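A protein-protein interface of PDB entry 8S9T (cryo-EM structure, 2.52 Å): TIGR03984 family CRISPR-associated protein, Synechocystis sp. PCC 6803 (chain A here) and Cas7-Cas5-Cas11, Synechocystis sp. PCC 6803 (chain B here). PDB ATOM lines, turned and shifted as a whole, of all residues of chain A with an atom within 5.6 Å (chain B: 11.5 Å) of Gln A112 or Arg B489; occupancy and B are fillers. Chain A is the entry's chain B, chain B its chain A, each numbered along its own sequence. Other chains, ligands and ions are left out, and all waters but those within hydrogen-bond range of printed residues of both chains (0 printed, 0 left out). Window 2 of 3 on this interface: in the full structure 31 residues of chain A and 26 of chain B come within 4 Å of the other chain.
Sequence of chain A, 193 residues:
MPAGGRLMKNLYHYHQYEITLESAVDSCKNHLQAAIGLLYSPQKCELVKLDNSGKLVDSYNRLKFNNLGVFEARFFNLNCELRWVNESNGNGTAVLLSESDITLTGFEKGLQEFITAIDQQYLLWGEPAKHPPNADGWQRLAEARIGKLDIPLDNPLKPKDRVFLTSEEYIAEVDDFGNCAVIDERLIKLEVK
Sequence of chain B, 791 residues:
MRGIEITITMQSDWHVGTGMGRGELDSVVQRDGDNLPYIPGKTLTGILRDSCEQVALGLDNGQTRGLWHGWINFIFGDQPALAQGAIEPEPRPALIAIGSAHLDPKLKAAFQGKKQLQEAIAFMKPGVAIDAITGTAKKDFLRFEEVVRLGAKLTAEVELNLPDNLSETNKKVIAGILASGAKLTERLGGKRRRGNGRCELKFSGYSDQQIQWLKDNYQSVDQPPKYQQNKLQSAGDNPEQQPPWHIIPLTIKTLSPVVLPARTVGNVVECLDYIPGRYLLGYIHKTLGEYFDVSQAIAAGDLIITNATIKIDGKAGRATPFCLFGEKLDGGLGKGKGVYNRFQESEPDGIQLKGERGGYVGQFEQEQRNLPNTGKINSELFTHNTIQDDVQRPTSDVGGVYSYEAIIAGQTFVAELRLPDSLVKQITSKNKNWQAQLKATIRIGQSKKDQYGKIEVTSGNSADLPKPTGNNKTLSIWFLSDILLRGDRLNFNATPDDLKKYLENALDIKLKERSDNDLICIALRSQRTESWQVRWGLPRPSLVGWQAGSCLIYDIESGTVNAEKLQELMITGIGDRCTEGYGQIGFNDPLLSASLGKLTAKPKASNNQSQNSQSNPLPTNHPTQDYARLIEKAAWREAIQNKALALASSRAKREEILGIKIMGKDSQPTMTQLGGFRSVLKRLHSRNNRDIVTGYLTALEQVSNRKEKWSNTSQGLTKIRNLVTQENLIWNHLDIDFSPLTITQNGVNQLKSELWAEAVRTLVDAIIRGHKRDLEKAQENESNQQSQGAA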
ATOM      1  N   LYS A   9       4.746  19.017 -24.646  1.00  0.00           N
ATOM      2  CA  LYS A   9       3.383  18.954 -24.125  1.00  0.00           C
ATOM      3  C   LYS A   9       3.116  20.165 -23.232  1.00  0.00           C
ATOM      4  O   LYS A   9       3.736  20.305 -22.187  1.00  0.00           O
ATOM      5  CB  LYS A   9       3.196  17.645 -23.362  1.00  0.00           C
ATOM      6  CG  LYS A   9       1.837  17.428 -22.789  1.00  0.00           C
ATOM      7  CD  LYS A   9       0.807  17.167 -23.867  1.00  0.00           C
ATOM      8  CE  LYS A   9       0.985  15.805 -24.503  1.00  0.00           C
ATOM      9  NZ  LYS A   9      -0.057  15.563 -25.538  1.00  0.00           N
ATOM     10  N   ASN A  10       2.193  21.036 -23.634  1.00  0.00           N
ATOM     11  CA  ASN A  10       1.962  22.297 -22.940  1.00  0.00           C
ATOM     12  C   ASN A  10       0.521  22.410 -22.470  1.00  0.00           C
ATOM     13  O   ASN A  10      -0.406  21.993 -23.168  1.00  0.00           O
ATOM     14  CB  ASN A  10       2.298  23.494 -23.828  1.00  0.00           C
ATOM     15  CG  ASN A  10       3.719  23.461 -24.340  1.00  0.00           C
ATOM     16  OD1 ASN A  10       4.633  23.022 -23.647  1.00  0.00           O
ATOM     17  ND2 ASN A  10       3.915  23.925 -25.565  1.00  0.00           N
ATOM     18  N   LEU A  11       0.346  22.985 -21.285  1.00  0.00           N
ATOM     19  CA  LEU A  11      -0.935  23.507 -20.832  1.00  0.00           C
ATOM     20  C   LEU A  11      -0.950  25.012 -21.074  1.00  0.00           C
ATOM     21  O   LEU A  11      -0.216  25.757 -20.419  1.00  0.00           O
ATOM     22  CB  LEU A  11      -1.147  23.194 -19.355  1.00  0.00           C
ATOM     23  CG  LEU A  11      -2.416  23.725 -18.698  1.00  0.00           C
ATOM     24  CD1 LEU A  11      -3.636  23.015 -19.242  1.00  0.00           C
ATOM     25  CD2 LEU A  11      -2.328  23.582 -17.193  1.00  0.00           C
ATOM     26  N   TYR A  12      -1.799  25.457 -21.995  1.00  0.00           N
ATOM     27  CA  TYR A  12      -1.928  26.873 -22.284  1.00  0.00           C
ATOM     28  C   TYR A  12      -2.890  27.536 -21.312  1.00  0.00           C
ATOM     29  O   TYR A  12      -3.941  26.987 -20.986  1.00  0.00           O
ATOM     30  CB  TYR A  12      -2.402  27.066 -23.721  1.00  0.00           C
ATOM     31  CG  TYR A  12      -1.476  26.435 -24.733  1.00  0.00           C
ATOM     32  CD1 TYR A  12      -0.366  27.118 -25.199  1.00  0.00           C
ATOM     33  CD2 TYR A  12      -1.695  25.152 -25.202  1.00  0.00           C
ATOM     34  CE1 TYR A  12       0.479  26.554 -26.112  1.00  0.00           C
ATOM     35  CE2 TYR A  12      -0.849  24.576 -26.112  1.00  0.00           C
ATOM     36  CZ  TYR A  12       0.236  25.282 -26.568  1.00  0.00           C
ATOM     37  OH  TYR A  12       1.095  24.707 -27.476  1.00  0.00           O
ATOM     38  N   HIS A  13      -2.510  28.719 -20.838  1.00  0.00           N
ATOM     39  CA  HIS A  13      -3.327  29.519 -19.939  1.00  0.00           C
ATOM     40  C   HIS A  13      -3.364  30.971 -20.392  1.00  0.00           C
ATOM     41  O   HIS A  13      -2.350  31.526 -20.820  1.00  0.00           O
ATOM     42  CB  HIS A  13      -2.822  29.415 -18.505  1.00  0.00           C
ATOM     43  CG  HIS A  13      -1.411  29.866 -18.324  1.00  0.00           C
ATOM     44  ND1 HIS A  13      -1.070  31.180 -18.093  1.00  0.00           N
ATOM     45  CD2 HIS A  13      -0.251  29.170 -18.318  1.00  0.00           C
ATOM     46  CE1 HIS A  13       0.239  31.276 -17.963  1.00  0.00           C
ATOM     47  NE2 HIS A  13       0.760  30.071 -18.095  1.00  0.00           N
ATOM     48  N   ARG A  83     -11.667  30.468 -15.158  1.00  0.00           N
ATOM     49  CA  ARG A  83     -11.687  30.816 -13.745  1.00  0.00           C
ATOM     50  C   ARG A  83     -11.700  32.327 -13.593  1.00  0.00           C
ATOM     51  O   ARG A  83     -10.970  33.029 -14.290  1.00  0.00           O
ATOM     52  CB  ARG A  83     -10.469  30.253 -13.045  1.00  0.00           C
ATOM     53  CG  ARG A  83     -10.365  28.778 -13.154  1.00  0.00           C
ATOM     54  CD  ARG A  83      -9.040  28.314 -12.672  1.00  0.00           C
ATOM     55  NE  ARG A  83      -8.924  26.874 -12.808  1.00  0.00           N
ATOM     56  CZ  ARG A  83      -7.793  26.205 -12.666  1.00  0.00           C
ATOM     57  NH1 ARG A  83      -6.670  26.855 -12.416  1.00  0.00           N
ATOM     58  NH2 ARG A  83      -7.785  24.892 -12.809  1.00  0.00           N
ATOM     59  N   VAL A  95      -8.706  33.745 -15.702  1.00  0.00           N
ATOM     60  CA  VAL A  95      -7.743  32.834 -16.308  1.00  0.00           C
ATOM     61  C   VAL A  95      -8.532  31.729 -16.982  1.00  0.00           C
ATOM     62  O   VAL A  95      -9.392  31.105 -16.353  1.00  0.00           O
ATOM     63  CB  VAL A  95      -6.777  32.219 -15.273  1.00  0.00           C
ATOM     64  CG1 VAL A  95      -5.842  31.229 -15.942  1.00  0.00           C
ATOM     65  CG2 VAL A  95      -5.995  33.277 -14.551  1.00  0.00           C
ATOM     66  N   LEU A  97      -8.017  28.043 -18.818  1.00  0.00           N
ATOM     67  CA  LEU A  97      -7.099  26.932 -19.022  1.00  0.00           C
ATOM     68  C   LEU A  97      -7.559  26.077 -20.187  1.00  0.00           C
ATOM     69  O   LEU A  97      -8.721  25.675 -20.242  1.00  0.00           O
ATOM     70  CB  LEU A  97      -6.995  26.055 -17.775  1.00  0.00           C
ATOM     71  CG  LEU A  97      -6.465  26.647 -16.484  1.00  0.00           C
ATOM     72  CD1 LEU A  97      -6.116  25.503 -15.558  1.00  0.00           C
ATOM     73  CD2 LEU A  97      -5.266  27.517 -16.743  1.00  0.00           C
ATOM     74  N   GLY A 110      -0.207  32.430 -21.982  1.00  0.00           N
ATOM     75  CA  GLY A 110       0.989  31.779 -21.492  1.00  0.00           C
ATOM     76  C   GLY A 110       0.863  30.279 -21.666  1.00  0.00           C
ATOM     77  O   GLY A 110      -0.134  29.785 -22.193  1.00  0.00           O
ATOM     78  N   LEU A 111       1.897  29.564 -21.240  1.00  0.00           N
ATOM     79  CA  LEU A 111       1.843  28.112 -21.272  1.00  0.00           C
ATOM     80  C   LEU A 111       2.724  27.543 -20.175  1.00  0.00           C
ATOM     81  O   LEU A 111       3.635  28.204 -19.677  1.00  0.00           O
ATOM     82  CB  LEU A 111       2.243  27.574 -22.653  1.00  0.00           C
ATOM     83  CG  LEU A 111       3.646  27.819 -23.218  1.00  0.00           C
ATOM     84  CD1 LEU A 111       4.657  26.764 -22.786  1.00  0.00           C
ATOM     85  CD2 LEU A 111       3.566  27.883 -24.725  1.00  0.00           C
ATOM     86  N   GLN A 112       2.433  26.299 -19.805  1.00  0.00           N
ATOM     87  CA  GLN A 112       3.303  25.490 -18.963  1.00  0.00           C
ATOM     88  C   GLN A 112       3.560  24.156 -19.633  1.00  0.00           C
ATOM     89  O   GLN A 112       2.624  23.505 -20.098  1.00  0.00           O
ATOM     90  CB  GLN A 112       2.684  25.234 -17.596  1.00  0.00           C
ATOM     91  CG  GLN A 112       2.559  26.427 -16.712  1.00  0.00           C
ATOM     92  CD  GLN A 112       1.991  26.049 -15.371  1.00  0.00           C
ATOM     93  OE1 GLN A 112       0.789  25.839 -15.235  1.00  0.00           O
ATOM     94  NE2 GLN A 112       2.858  25.924 -14.373  1.00  0.00           N
ATOM     95  N   GLU A 113       4.815  23.737 -19.660  1.00  0.00           N
ATOM     96  CA  GLU A 113       5.097  22.354 -19.999  1.00  0.00           C
ATOM     97  C   GLU A 113       4.647  21.463 -18.852  1.00  0.00           C
ATOM     98  O   GLU A 113       4.798  21.814 -17.681  1.00  0.00           O
ATOM     99  CB  GLU A 113       6.585  22.170 -20.280  1.00  0.00           C
ATOM    100  CG  GLU A 113       7.082  22.994 -21.451  1.00  0.00           C
ATOM    101  CD  GLU A 113       8.525  22.706 -21.798  1.00  0.00           C
ATOM    102  OE1 GLU A 113       8.911  21.520 -21.782  1.00  0.00           O
ATOM    103  OE2 GLU A 113       9.274  23.664 -22.078  1.00  0.00           O
ATOM    104  N   PHE A 114       4.067  20.321 -19.187  1.00  0.00           N
ATOM    105  CA  PHE A 114       3.786  19.297 -18.196  1.00  0.00           C
ATOM    106  C   PHE A 114       4.195  17.941 -18.744  1.00  0.00           C
ATOM    107  O   PHE A 114       4.097  17.686 -19.946  1.00  0.00           O
ATOM    108  CB  PHE A 114       2.311  19.362 -17.729  1.00  0.00           C
ATOM    109  CG  PHE A 114       1.300  19.006 -18.778  1.00  0.00           C
ATOM    110  CD1 PHE A 114       0.893  17.703 -18.966  1.00  0.00           C
ATOM    111  CD2 PHE A 114       0.772  19.988 -19.591  1.00  0.00           C
ATOM    112  CE1 PHE A 114      -0.032  17.397 -19.921  1.00  0.00           C
ATOM    113  CE2 PHE A 114      -0.143  19.683 -20.549  1.00  0.00           C
ATOM    114  CZ  PHE A 114      -0.550  18.386 -20.713  1.00  0.00           C
ATOM    115  N   ILE A 183       0.827  20.444 -11.185  1.00  0.00           N
ATOM    116  CA  ILE A 183       0.880  21.897 -11.187  1.00  0.00           C
ATOM    117  C   ILE A 183      -0.495  22.528 -11.317  1.00  0.00           C
ATOM    118  O   ILE A 183      -0.694  23.664 -10.878  1.00  0.00           O
ATOM    119  CB  ILE A 183       1.789  22.383 -12.316  1.00  0.00           C
ATOM    120  CG1 ILE A 183       1.434  21.636 -13.601  1.00  0.00           C
ATOM    121  CG2 ILE A 183       3.233  22.174 -11.924  1.00  0.00           C
ATOM    122  CD1 ILE A 183       1.811  22.345 -14.859  1.00  0.00           C
ATOM    123  N   ASP A 184      -1.450  21.826 -11.912  1.00  0.00           N
ATOM    124  CA  ASP A 184      -2.811  22.327 -11.957  1.00  0.00           C
ATOM    125  C   ASP A 184      -3.751  21.158 -12.182  1.00  0.00           C
ATOM    126  O   ASP A 184      -3.334  20.060 -12.547  1.00  0.00           O
ATOM    127  CB  ASP A 184      -2.968  23.376 -13.058  1.00  0.00           C
ATOM    128  CG  ASP A 184      -3.946  24.453 -12.690  1.00  0.00           C
ATOM    129  OD1 ASP A 184      -4.884  24.166 -11.927  1.00  0.00           O
ATOM    130  OD2 ASP A 184      -3.771  25.593 -13.156  1.00  0.00           O
ATOM    131  N   LEU B 485      -2.935  32.321  -0.978  1.00  0.00           N
ATOM    132  CA  LEU B 485      -2.606  33.005  -2.215  1.00  0.00           C
ATOM    133  C   LEU B 485      -3.104  32.204  -3.405  1.00  0.00           C
ATOM    134  O   LEU B 485      -2.961  30.982  -3.446  1.00  0.00           O
ATOM    135  CB  LEU B 485      -1.106  33.244  -2.364  1.00  0.00           C
ATOM    136  CG  LEU B 485      -0.481  34.489  -1.751  1.00  0.00           C
ATOM    137  CD1 LEU B 485       0.974  34.546  -2.122  1.00  0.00           C
ATOM    138  CD2 LEU B 485      -1.185  35.737  -2.229  1.00  0.00           C
ATOM    139  N   ARG B 486      -3.682  32.907  -4.371  1.00  0.00           N
ATOM    140  CA  ARG B 486      -3.892  32.345  -5.694  1.00  0.00           C
ATOM    141  C   ARG B 486      -2.558  32.173  -6.402  1.00  0.00           C
ATOM    142  O   ARG B 486      -1.706  33.062  -6.372  1.00  0.00           O
ATOM    143  CB  ARG B 486      -4.777  33.259  -6.534  1.00  0.00           C
ATOM    144  CG  ARG B 486      -6.134  33.563  -5.980  1.00  0.00           C
ATOM    145  CD  ARG B 486      -6.986  32.350  -5.934  1.00  0.00           C
ATOM    146  NE  ARG B 486      -8.288  32.647  -5.368  1.00  0.00           N
ATOM    147  CZ  ARG B 486      -9.355  31.886  -5.539  1.00  0.00           C
ATOM    148  NH1 ARG B 486      -9.277  30.800  -6.284  1.00  0.00           N
ATOM    149  NH2 ARG B 486     -10.498  32.222  -4.983  1.00  0.00           N
ATOM    150  N   GLY B 487      -2.372  31.036  -7.038  1.00  0.00           N
ATOM    151  CA  GLY B 487      -1.376  30.960  -8.077  1.00  0.00           C
ATOM    152  C   GLY B 487      -1.764  31.843  -9.247  1.00  0.00           C
ATOM    153  O   GLY B 487      -2.843  32.430  -9.295  1.00  0.00           O
ATOM    154  N   ASP B 488      -0.857  31.961 -10.212  1.00  0.00           N
ATOM    155  CA  ASP B 488      -1.214  32.737 -11.390  1.00  0.00           C
ATOM    156  C   ASP B 488      -2.281  32.076 -12.258  1.00  0.00           C
ATOM    157  O   ASP B 488      -2.780  32.726 -13.180  1.00  0.00           O
ATOM    158  CB  ASP B 488       0.035  33.033 -12.220  1.00  0.00           C
ATOM    159  CG  ASP B 488       0.701  31.783 -12.736  1.00  0.00           C
ATOM    160  OD1 ASP B 488       0.300  30.678 -12.322  1.00  0.00           O
ATOM    161  OD2 ASP B 488       1.626  31.903 -13.569  1.00  0.00           O
ATOM    162  N   ARG B 489      -2.671  30.831 -11.985  1.00  0.00           N
ATOM    163  CA  ARG B 489      -3.889  30.278 -12.558  1.00  0.00           C
ATOM    164  C   ARG B 489      -5.070  30.326 -11.598  1.00  0.00           C
ATOM    165  O   ARG B 489      -6.062  29.632 -11.827  1.00  0.00           O
ATOM    166  CB  ARG B 489      -3.695  28.856 -13.094  1.00  0.00           C
ATOM    167  CG  ARG B 489      -2.810  28.726 -14.339  1.00  0.00           C
ATOM    168  CD  ARG B 489      -1.342  28.530 -14.075  1.00  0.00           C
ATOM    169  NE  ARG B 489      -1.115  27.275 -13.363  1.00  0.00           N
ATOM    170  CZ  ARG B 489      -0.057  27.015 -12.602  1.00  0.00           C
ATOM    171  NH1 ARG B 489       0.860  27.945 -12.385  1.00  0.00           N
ATOM    172  NH2 ARG B 489       0.052  25.838 -12.006  1.00  0.00           N
ATOM    173  N   LEU B 490      -4.962  31.088 -10.509  1.00  0.00           N
ATOM    174  CA  LEU B 490      -6.028  31.293  -9.529  1.00  0.00           C
ATOM    175  C   LEU B 490      -6.452  30.037  -8.788  1.00  0.00           C
ATOM    176  O   LEU B 490      -7.405  30.077  -8.013  1.00  0.00           O
ATOM    177  CB  LEU B 490      -7.264  31.920 -10.183  1.00  0.00           C
ATOM    178  CG  LEU B 490      -7.150  33.204 -11.000  1.00  0.00           C
ATOM    179  CD1 LEU B 490      -8.490  33.570 -11.576  1.00  0.00           C
ATOM    180  CD2 LEU B 490      -6.638  34.316 -10.129  1.00  0.00           C
ATOM    181  N   ASN B 491      -5.801  28.913  -9.043  1.00  0.00           N
ATOM    182  CA  ASN B 491      -5.833  27.841  -8.067  1.00  0.00           C
ATOM    183  C   ASN B 491      -5.085  28.282  -6.815  1.00  0.00           C
ATOM    184  O   ASN B 491      -4.270  29.204  -6.845  1.00  0.00           O
ATOM    185  CB  ASN B 491      -5.212  26.570  -8.647  1.00  0.00           C
ATOM    186  CG  ASN B 491      -3.754  26.743  -8.995  1.00  0.00           C
ATOM    187  OD1 ASN B 491      -3.378  27.663  -9.711  1.00  0.00           O
ATOM    188  ND2 ASN B 491      -2.917  25.851  -8.485  1.00  0.00           N
ATOM    189  N   PHE B 492      -5.364  27.629  -5.700  1.00  0.00           N
ATOM    190  CA  PHE B 492      -4.526  27.964  -4.565  1.00  0.00           C
ATOM    191  C   PHE B 492      -3.191  27.241  -4.691  1.00  0.00           C
ATOM    192  O   PHE B 492      -3.069  26.221  -5.367  1.00  0.00           O
ATOM    193  CB  PHE B 492      -5.255  27.678  -3.263  1.00  0.00           C
ATOM    194  CG  PHE B 492      -6.220  28.757  -2.911  1.00  0.00           C
ATOM    195  CD1 PHE B 492      -5.770  29.963  -2.418  1.00  0.00           C
ATOM    196  CD2 PHE B 492      -7.567  28.598  -3.142  1.00  0.00           C
ATOM    197  CE1 PHE B 492      -6.647  30.967  -2.129  1.00  0.00           C
ATOM    198  CE2 PHE B 492      -8.446  29.604  -2.849  1.00  0.00           C
ATOM    199  CZ  PHE B 492      -7.984  30.787  -2.341  1.00  0.00           C
ATOM    200  N   ASN B 493      -2.187  27.760  -4.000  1.00  0.00           N
ATOM    201  CA  ASN B 493      -0.822  27.493  -4.421  1.00  0.00           C
ATOM    202  C   ASN B 493       0.118  27.435  -3.223  1.00  0.00           C
ATOM    203  O   ASN B 493      -0.195  27.909  -2.127  1.00  0.00           O
ATOM    204  CB  ASN B 493      -0.370  28.562  -5.422  1.00  0.00           C
ATOM    205  CG  ASN B 493       1.092  28.514  -5.706  1.00  0.00           C
ATOM    206  OD1 ASN B 493       1.882  29.199  -5.058  1.00  0.00           O
ATOM    207  ND2 ASN B 493       1.476  27.703  -6.679  1.00  0.00           N
ATOM    208  N   ALA B 494       1.281  26.831  -3.457  1.00  0.00           N
ATOM    209  CA  ALA B 494       2.378  26.764  -2.503  1.00  0.00           C
ATOM    210  C   ALA B 494       3.707  27.104  -3.177  1.00  0.00           C
ATOM    211  O   ALA B 494       4.683  26.358  -3.079  1.00  0.00           O
ATOM    212  CB  ALA B 494       2.446  25.387  -1.851  1.00  0.00           C
ATOM    213  N   THR B 495       3.768  28.236  -3.878  1.00  0.00           N
ATOM    214  CA  THR B 495       5.024  28.691  -4.486  1.00  0.00           C
ATOM    215  C   THR B 495       5.460  30.029  -3.909  1.00  0.00           C
ATOM    216  O   THR B 495       4.848  31.065  -4.225  1.00  0.00           O
ATOM    217  CB  THR B 495       4.913  28.806  -6.005  1.00  0.00           C
ATOM    218  OG1 THR B 495       4.386  27.595  -6.555  1.00  0.00           O
ATOM    219  CG2 THR B 495       6.278  29.067  -6.599  1.00  0.00           C
ATOM    220  N   PRO B 496       6.522  30.063  -3.099  1.00  0.00           N
ATOM    221  CA  PRO B 496       6.895  31.310  -2.419  1.00  0.00           C
ATOM    222  C   PRO B 496       7.377  32.407  -3.343  1.00  0.00           C
ATOM    223  O   PRO B 496       7.358  33.574  -2.939  1.00  0.00           O
ATOM    224  CB  PRO B 496       8.000  30.866  -1.456  1.00  0.00           C
ATOM    225  CG  PRO B 496       8.512  29.609  -2.013  1.00  0.00           C
ATOM    226  CD  PRO B 496       7.362  28.936  -2.676  1.00  0.00           C
ATOM    227  N   ASP B 497       7.845  32.082  -4.548  1.00  0.00           N
ATOM    228  CA  ASP B 497       8.152  33.124  -5.522  1.00  0.00           C
ATOM    229  C   ASP B 497       6.931  33.960  -5.866  1.00  0.00           C
ATOM    230  O   ASP B 497       7.066  35.126  -6.248  1.00  0.00           O
ATOM    231  CB  ASP B 497       8.736  32.511  -6.793  1.00  0.00           C
ATOM    232  CG  ASP B 497      10.061  31.824  -6.551  1.00  0.00           C
ATOM    233  OD1 ASP B 497      10.685  32.088  -5.503  1.00  0.00           O
ATOM    234  OD2 ASP B 497      10.484  31.025  -7.412  1.00  0.00           O
ATOM    235  N   ASP B 498       5.733  33.387  -5.753  1.00  0.00           N
ATOM    236  CA  ASP B 498       4.522  34.171  -5.969  1.00  0.00           C
ATOM    237  C   ASP B 498       4.289  35.156  -4.833  1.00  0.00           C
ATOM    238  O   ASP B 498       3.831  36.280  -5.064  1.00  0.00           O
ATOM    239  CB  ASP B 498       3.318  33.251  -6.132  1.00  0.00           C
ATOM    240  CG  ASP B 498       3.465  32.306  -7.300  1.00  0.00           C
ATOM    241  OD1 ASP B 498       4.336  32.552  -8.157  1.00  0.00           O
ATOM    242  OD2 ASP B 498       2.693  31.332  -7.382  1.00  0.00           O
ATOM    243  N   LYS B 501       6.797  37.906  -5.451  1.00  0.00           N
ATOM    244  CA  LYS B 501       6.208  38.797  -6.445  1.00  0.00           C
ATOM    245  C   LYS B 501       5.076  39.626  -5.861  1.00  0.00           C
ATOM    246  O   LYS B 501       4.976  40.825  -6.133  1.00  0.00           O
ATOM    247  CB  LYS B 501       5.712  37.990  -7.638  1.00  0.00           C
ATOM    248  CG  LYS B 501       6.819  37.526  -8.555  1.00  0.00           C
ATOM    249  CD  LYS B 501       6.276  36.700  -9.702  1.00  0.00           C
ATOM    250  CE  LYS B 501       7.351  36.458 -10.742  1.00  0.00           C
ATOM    251  NZ  LYS B 501       8.403  35.534 -10.237  1.00  0.00           N
ATOM    252  N   ASP B 576      -5.964  36.250  -0.194  1.00  0.00           N
ATOM    253  CA  ASP B 576      -7.396  36.012  -0.271  1.00  0.00           C
ATOM    254  C   ASP B 576      -8.042  35.894   1.108  1.00  0.00           C
ATOM    255  O   ASP B 576      -7.411  35.481   2.079  1.00  0.00           O
ATOM    256  CB  ASP B 576      -7.661  34.742  -1.085  1.00  0.00           C
ATOM    257  CG  ASP B 576      -8.914  34.843  -1.955  1.00  0.00           C
ATOM    258  OD1 ASP B 576      -9.669  35.834  -1.847  1.00  0.00           O
ATOM    259  OD2 ASP B 576      -9.145  33.914  -2.757  1.00  0.00           O
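The backbone carbonyl oxygen (O) of Arg B489 sits at hydrogen-bond distance from the guanidinium group (NH1) of Arg A83 (2.9 Å). The guanidinium group of Arg B489 lies close to the side-chain amide oxygen of Gln A112. The side-chain carboxylate (OD2) of Asp A184 is in salt-bridge range of the guanidinium group (NE) of Arg B489, at 3.2 Å. NH2 of Arg B489 lies within hydrogen-bond range of O of Ile A183 (2.6 Å).
The backbone carbonyl oxygen (O) of Gln A112 lies within hydrogen-bond range of the backbone NH (N) of Leu A11 (2.6 Å). NH1 of Arg B486 lies within hydrogen-bond range of O of Leu B490 (2.6 Å). OD1 of Asp A184 lies within salt-bridge range of NH2 of Arg A83 (3.1 Å). N of Arg A83 sits at hydrogen-bond distance from O of Val A95 (2.6 Å). The side-chain carboxylate (OD1) of Asp B488 lies within salt-bridge range of the guanidinium group (NH1) of Arg B489 (2.8 Å).
Among the printed residues, merely in contact across the chains: Arg A83 with Leu B490 (3.7 Å), Val A95 with Asp B488 (3.5 Å), Val A95 with Leu B490 (3.7 Å), Leu A97 with Arg B489 (3.6 Å) and Ile A183 with Asn B491 (3.9 Å).
Of chain B, only Arg B489 (3.0 Å) comes within 4 Å of Gln A112. Arg B489 touches five residues of chain A. Asn A10 touches none of the printed residues of chain B. No residue of chain B comes within 4 Å of Leu A11. No residue of chain B comes within 4 Å of His A13. Of chain B, only Arg B489 (2.9 Å) and Leu B490 (3.7 Å) come within 4 Å of Arg A83. Val A95 touches just these residues of chain B: Asp B488 (3.5 Å) and Leu B490 (3.7 Å). No residue of chain B comes within 4 Å of Gly A110. No residue of chain B comes within 4 Å of Leu A111. No residue of chain B comes within 4 Å of Glu A113. Of chain B, only Arg B489 (3.2 Å) comes within 4 Å of Asp A184. Of the printed residues of chain A, Asn B491 touches Ile A183. Printed residues of chain A within 4 Å of Leu B490: Arg A83 (3.7 Å) and Val A95 (3.7 Å). Of the printed residues of chain B, Leu A97 touches Arg B489 (3.6 Å). Of the printed residues of chain A, Asp B488 touches Val A95. Phe B492 touches none of the printed residues of chain A. Asp B576 touches none of the printed residues of chain A. The nearest residue of chain B that does not touch Gln A112 is Asp B488 (5.7 Å). The nearest residue of chain A that does not touch Arg B489 is Val A95 (4.02 Å).
Of the 16 printed residues of chain B, 4 touch a printed residue of chain A. Printed residues of chain B that touch a printed residue of chain A: Asp B488, Arg B489, Leu B490 and Asn B491. Hydrophobic or aromatic side chains of chain B that line the printed part of chain A: Leu B490. Of the 15 printed residues of chain A, 6 touch a printed residue of chain B. Printed residues of chain A that touch a printed residue of chain B: Arg A83, Val A95, Leu A97, Gln A112, Ile A183 and Asp A184. Hydrophobic or aromatic side chains of chain A that line the printed part of chain B: Val A95, Leu A97 and Ile A183.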
